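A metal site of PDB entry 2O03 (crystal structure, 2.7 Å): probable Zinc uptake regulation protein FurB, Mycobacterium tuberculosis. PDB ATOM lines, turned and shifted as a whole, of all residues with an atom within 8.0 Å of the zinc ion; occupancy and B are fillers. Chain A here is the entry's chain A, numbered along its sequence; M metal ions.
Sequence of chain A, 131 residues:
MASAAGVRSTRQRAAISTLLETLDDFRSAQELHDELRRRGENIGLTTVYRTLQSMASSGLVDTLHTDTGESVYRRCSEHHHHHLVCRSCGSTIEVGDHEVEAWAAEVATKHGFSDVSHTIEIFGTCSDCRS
Four residues have an atom within 4 Å of the zinc ion: Asp 62, Cys 76, His 81 and His 83.
N of Asp 62 sits at hydrogen-bond distance from O of Arg 74, 2.9 Å away.
A ring nitrogen (ND1) of His 81 sits at hydrogen-bond distance from the backbone carbonyl oxygen of His 79 (2.8 Å).
The backbone carbonyl oxygen (O) of Leu 60 is in hydrogen-bond range of the backbone NH (N) of Cys 76 (3.3 Å).
The zinc ion is bound by OD2 of Asp 62 (2.0 Å), NE2 of His 83 (2.0 Å), NE2 of His 81 (2.1 Å) and SG of Cys 76 (2.3 Å).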
ATOM      1  N   PHE A  26      22.374 -16.602  28.586  1.00  0.00           N
ATOM      2  CA  PHE A  26      23.483 -17.563  28.710  1.00  0.00           C
ATOM      3  C   PHE A  26      23.049 -19.033  28.692  1.00  0.00           C
ATOM      4  O   PHE A  26      22.146 -19.413  29.436  1.00  0.00           O
ATOM      5  CB  PHE A  26      24.233 -17.297  30.019  1.00  0.00           C
ATOM      6  CG  PHE A  26      25.201 -16.167  29.930  1.00  0.00           C
ATOM      7  CD1 PHE A  26      26.504 -16.378  29.514  1.00  0.00           C
ATOM      8  CD2 PHE A  26      24.807 -14.874  30.263  1.00  0.00           C
ATOM      9  CE1 PHE A  26      27.398 -15.325  29.440  1.00  0.00           C
ATOM     10  CE2 PHE A  26      25.711 -13.809  30.195  1.00  0.00           C
ATOM     11  CZ  PHE A  26      27.016 -14.051  29.775  1.00  0.00           C
ATOM     12  N   GLY A  59      36.141 -13.184  20.806  1.00  0.00           N
ATOM     13  CA  GLY A  59      35.296 -12.079  21.187  1.00  0.00           C
ATOM     14  C   GLY A  59      33.990 -11.983  20.427  1.00  0.00           C
ATOM     15  O   GLY A  59      33.541 -10.876  20.131  1.00  0.00           O
ATOM     16  N   LEU A  60      33.396 -13.125  20.112  1.00  0.00           N
ATOM     17  CA  LEU A  60      32.086 -13.172  19.505  1.00  0.00           C
ATOM     18  C   LEU A  60      31.052 -13.545  20.543  1.00  0.00           C
ATOM     19  O   LEU A  60      29.974 -12.971  20.562  1.00  0.00           O
ATOM     20  CB  LEU A  60      32.044 -14.139  18.318  1.00  0.00           C
ATOM     21  CG  LEU A  60      32.871 -13.721  17.086  1.00  0.00           C
ATOM     22  CD1 LEU A  60      33.480 -14.942  16.398  1.00  0.00           C
ATOM     23  CD2 LEU A  60      32.053 -12.844  16.089  1.00  0.00           C
ATOM     24  N   VAL A  61      31.370 -14.510  21.416  1.00  0.00           N
ATOM     25  CA  VAL A  61      30.519 -14.778  22.595  1.00  0.00           C
ATOM     26  C   VAL A  61      31.194 -14.392  23.925  1.00  0.00           C
ATOM     27  O   VAL A  61      32.415 -14.392  24.046  1.00  0.00           O
ATOM     28  CB  VAL A  61      30.025 -16.268  22.703  1.00  0.00           C
ATOM     29  CG1 VAL A  61      29.490 -16.796  21.397  1.00  0.00           C
ATOM     30  CG2 VAL A  61      31.113 -17.183  23.285  1.00  0.00           C
ATOM     31  N   ASP A  62      30.369 -14.071  24.909  1.00  0.00           N
ATOM     32  CA  ASP A  62      30.814 -13.841  26.269  1.00  0.00           C
ATOM     33  C   ASP A  62      30.555 -15.089  27.117  1.00  0.00           C
ATOM     34  O   ASP A  62      29.658 -15.865  26.805  1.00  0.00           O
ATOM     35  CB  ASP A  62      30.049 -12.671  26.858  1.00  0.00           C
ATOM     36  CG  ASP A  62      30.414 -11.370  26.193  1.00  0.00           C
ATOM     37  OD1 ASP A  62      31.316 -11.349  25.317  1.00  0.00           O
ATOM     38  OD2 ASP A  62      29.797 -10.356  26.553  1.00  0.00           O
ATOM     39  N   THR A  63      31.304 -15.257  28.186  1.00  0.00           N
ATOM     40  CA  THR A  63      31.228 -16.480  28.953  1.00  0.00           C
ATOM     41  C   THR A  63      31.097 -16.274  30.477  1.00  0.00           C
ATOM     42  O   THR A  63      31.482 -15.213  31.010  1.00  0.00           O
ATOM     43  CB  THR A  63      32.434 -17.394  28.576  1.00  0.00           C
ATOM     44  OG1 THR A  63      32.061 -18.774  28.701  1.00  0.00           O
ATOM     45  CG2 THR A  63      33.647 -17.109  29.432  1.00  0.00           C
ATOM     46  N   ARG A  74      26.848 -16.600  25.447  1.00  0.00           N
ATOM     47  CA  ARG A  74      25.879 -15.727  24.752  1.00  0.00           C
ATOM     48  C   ARG A  74      26.579 -14.892  23.658  1.00  0.00           C
ATOM     49  O   ARG A  74      27.669 -14.355  23.899  1.00  0.00           O
ATOM     50  CB  ARG A  74      25.145 -14.745  25.782  1.00  0.00           C
ATOM     51  N   ARG A  75      25.946 -14.702  22.481  1.00  0.00           N
ATOM     52  CA  ARG A  75      26.419 -13.658  21.527  1.00  0.00           C
ATOM     53  C   ARG A  75      26.422 -12.380  22.319  1.00  0.00           C
ATOM     54  O   ARG A  75      25.528 -12.190  23.119  1.00  0.00           O
ATOM     55  CB  ARG A  75      25.506 -13.503  20.299  1.00  0.00           C
ATOM     56  N   CYS A  76      27.426 -11.522  22.098  1.00  0.00           N
ATOM     57  CA  CYS A  76      27.633 -10.297  22.865  1.00  0.00           C
ATOM     58  C   CYS A  76      26.343  -9.487  23.045  1.00  0.00           C
ATOM     59  O   CYS A  76      25.555  -9.370  22.093  1.00  0.00           O
ATOM     60  CB  CYS A  76      28.725  -9.452  22.257  1.00  0.00           C
ATOM     61  SG  CYS A  76      29.483  -8.378  23.481  1.00  0.00           S
ATOM     62  N   SER A  77      26.160  -8.945  24.255  1.00  0.00           N
ATOM     63  CA  SER A  77      24.808  -8.678  24.860  1.00  0.00           C
ATOM     64  C   SER A  77      23.867  -7.545  24.347  1.00  0.00           C
ATOM     65  O   SER A  77      22.724  -7.443  24.837  1.00  0.00           O
ATOM     66  CB  SER A  77      24.927  -8.614  26.402  1.00  0.00           C
ATOM     67  N   GLU A  78      24.315  -6.709  23.397  1.00  0.00           N
ATOM     68  CA  GLU A  78      23.538  -5.555  22.840  1.00  0.00           C
ATOM     69  C   GLU A  78      23.331  -4.347  23.805  1.00  0.00           C
ATOM     70  O   GLU A  78      23.460  -3.195  23.393  1.00  0.00           O
ATOM     71  CB  GLU A  78      22.215  -5.989  22.164  1.00  0.00           C
ATOM     72  N   HIS A  79      23.032  -4.620  25.076  1.00  0.00           N
ATOM     73  CA  HIS A  79      23.034  -3.596  26.122  1.00  0.00           C
ATOM     74  C   HIS A  79      24.461  -3.202  26.509  1.00  0.00           C
ATOM     75  O   HIS A  79      25.340  -4.063  26.609  1.00  0.00           O
ATOM     76  CB  HIS A  79      22.247  -4.087  27.330  1.00  0.00           C
ATOM     77  CG  HIS A  79      20.777  -4.294  27.066  1.00  0.00           C
ATOM     78  ND1 HIS A  79      19.869  -3.249  27.022  1.00  0.00           N
ATOM     79  CD2 HIS A  79      20.054  -5.416  26.819  1.00  0.00           C
ATOM     80  CE1 HIS A  79      18.658  -3.721  26.772  1.00  0.00           C
ATOM     81  NE2 HIS A  79      18.743  -5.027  26.644  1.00  0.00           N
ATOM     82  N   HIS A  80      24.695  -1.902  26.711  1.00  0.00           N
ATOM     83  CA  HIS A  80      26.065  -1.373  26.951  1.00  0.00           C
ATOM     84  C   HIS A  80      26.760  -1.988  28.176  1.00  0.00           C
ATOM     85  O   HIS A  80      26.252  -1.898  29.290  1.00  0.00           O
ATOM     86  CB  HIS A  80      26.053   0.178  27.022  1.00  0.00           C
ATOM     87  CG  HIS A  80      27.366   0.789  27.382  1.00  0.00           C
ATOM     88  ND1 HIS A  80      28.153   1.458  26.468  1.00  0.00           N
ATOM     89  CD2 HIS A  80      28.015   0.894  28.577  1.00  0.00           C
ATOM     90  CE1 HIS A  80      29.240   1.921  27.077  1.00  0.00           C
ATOM     91  NE2 HIS A  80      29.182   1.594  28.346  1.00  0.00           N
ATOM     92  N   HIS A  81      27.906  -2.625  27.924  1.00  0.00           N
ATOM     93  CA  HIS A  81      28.740  -3.198  28.978  1.00  0.00           C
ATOM     94  C   HIS A  81      30.208  -3.168  28.579  1.00  0.00           C
ATOM     95  O   HIS A  81      30.538  -2.754  27.466  1.00  0.00           O
ATOM     96  CB  HIS A  81      28.303  -4.617  29.288  1.00  0.00           C
ATOM     97  CG  HIS A  81      28.497  -5.568  28.135  1.00  0.00           C
ATOM     98  ND1 HIS A  81      27.510  -5.811  27.204  1.00  0.00           N
ATOM     99  CD2 HIS A  81      29.556  -6.340  27.789  1.00  0.00           C
ATOM    100  CE1 HIS A  81      27.963  -6.683  26.319  1.00  0.00           C
ATOM    101  NE2 HIS A  81      29.197  -7.026  26.649  1.00  0.00           N
ATOM    102  N   HIS A  82      31.097  -3.594  29.478  1.00  0.00           N
ATOM    103  CA  HIS A  82      32.500  -3.776  29.136  1.00  0.00           C
ATOM    104  C   HIS A  82      32.955  -5.239  29.403  1.00  0.00           C
ATOM    105  O   HIS A  82      32.181  -6.054  29.927  1.00  0.00           O
ATOM    106  CB  HIS A  82      33.393  -2.732  29.869  1.00  0.00           C
ATOM    107  CG  HIS A  82      32.935  -1.310  29.698  1.00  0.00           C
ATOM    108  ND1 HIS A  82      33.184  -0.571  28.556  1.00  0.00           N
ATOM    109  CD2 HIS A  82      32.255  -0.488  30.533  1.00  0.00           C
ATOM    110  CE1 HIS A  82      32.661   0.641  28.686  1.00  0.00           C
ATOM    111  NE2 HIS A  82      32.103   0.723  29.887  1.00  0.00           N
ATOM    112  N   HIS A  83      34.204  -5.561  29.026  1.00  0.00           N
ATOM    113  CA  HIS A  83      34.722  -6.911  29.165  1.00  0.00           C
ATOM    114  C   HIS A  83      35.983  -7.052  29.978  1.00  0.00           C
ATOM    115  O   HIS A  83      36.876  -6.211  29.927  1.00  0.00           O
ATOM    116  CB  HIS A  83      35.037  -7.510  27.811  1.00  0.00           C
ATOM    117  CG  HIS A  83      33.917  -7.459  26.838  1.00  0.00           C
ATOM    118  ND1 HIS A  83      33.941  -6.671  25.716  1.00  0.00           N
ATOM    119  CD2 HIS A  83      32.734  -8.125  26.810  1.00  0.00           C
ATOM    120  CE1 HIS A  83      32.817  -6.824  25.038  1.00  0.00           C
ATOM    121  NE2 HIS A  83      32.077  -7.712  25.679  1.00  0.00           N
ATOM    122  N   LEU A  84      36.054  -8.174  30.696  1.00  0.00           N
ATOM    123  CA  LEU A  84      37.260  -8.706  31.313  1.00  0.00           C
ATOM    124  C   LEU A  84      37.866  -9.721  30.342  1.00  0.00           C
ATOM    125  O   LEU A  84      37.131 -10.526  29.766  1.00  0.00           O
ATOM    126  CB  LEU A  84      36.845  -9.416  32.583  1.00  0.00           C
ATOM    127  CG  LEU A  84      37.853 -10.192  33.414  1.00  0.00           C
ATOM    128  CD1 LEU A  84      39.031  -9.314  33.845  1.00  0.00           C
ATOM    129  CD2 LEU A  84      37.107 -10.722  34.612  1.00  0.00           C
ATOM    130  N   THR A  92      36.567 -14.189  27.206  1.00  0.00           N
ATOM    131  CA  THR A  92      35.906 -12.902  27.423  1.00  0.00           C
ATOM    132  C   THR A  92      34.715 -13.030  28.395  1.00  0.00           C
ATOM    133  O   THR A  92      33.783 -13.818  28.147  1.00  0.00           O
ATOM    134  CB  THR A  92      35.363 -12.291  26.100  1.00  0.00           C
ATOM    135  OG1 THR A  92      36.243 -12.587  25.012  1.00  0.00           O
ATOM    136  CG2 THR A  92      35.196 -10.807  26.235  1.00  0.00           C
ATOM    137  N   ILE A  93      34.748 -12.246  29.461  1.00  0.00           N
ATOM    138  CA  ILE A  93      33.687 -12.218  30.458  1.00  0.00           C
ATOM    139  C   ILE A  93      33.079 -10.838  30.460  1.00  0.00           C
ATOM    140  O   ILE A  93      33.812  -9.855  30.348  1.00  0.00           O
ATOM    141  CB  ILE A  93      34.231 -12.588  31.848  1.00  0.00           C
ATOM    142  CG1 ILE A  93      34.608 -14.058  31.849  1.00  0.00           C
ATOM    143  CG2 ILE A  93      33.192 -12.307  32.957  1.00  0.00           C
ATOM    144  CD1 ILE A  93      35.248 -14.541  33.097  1.00  0.00           C
ATOM    145  N   GLU A  94      31.745 -10.773  30.561  1.00  0.00           N
ATOM    146  CA  GLU A  94      31.000  -9.504  30.602  1.00  0.00           C
ATOM    147  C   GLU A  94      31.052  -8.874  31.988  1.00  0.00           C
ATOM    148  O   GLU A  94      30.816  -9.569  32.989  1.00  0.00           O
ATOM    149  CB  GLU A  94      29.539  -9.740  30.248  1.00  0.00           C
ATOM    150  CG  GLU A  94      28.668  -8.494  30.399  1.00  0.00           C
ATOM    151  CD  GLU A  94      27.236  -8.691  29.922  1.00  0.00           C
ATOM    152  OE1 GLU A  94      26.952  -9.679  29.199  1.00  0.00           O
ATOM    153  OE2 GLU A  94      26.395  -7.847  30.293  1.00  0.00           O
ATOM    154  N   VAL A  95      31.349  -7.581  32.029  1.00  0.00           N
ATOM    155  CA  VAL A  95      31.380  -6.795  33.286  1.00  0.00           C
ATOM    156  C   VAL A  95      30.731  -5.414  33.128  1.00  0.00           C
ATOM    157  O   VAL A  95      30.704  -4.854  32.032  1.00  0.00           O
ATOM    158  CB  VAL A  95      32.836  -6.628  33.891  1.00  0.00           C
ATOM    159  CG1 VAL A  95      33.413  -7.974  34.343  1.00  0.00           C
ATOM    160  CG2 VAL A  95      33.791  -5.933  32.909  1.00  0.00           C
HETATM  161 ZN    ZN M   1      30.245  -8.605  25.682  1.00  0.00          ZN
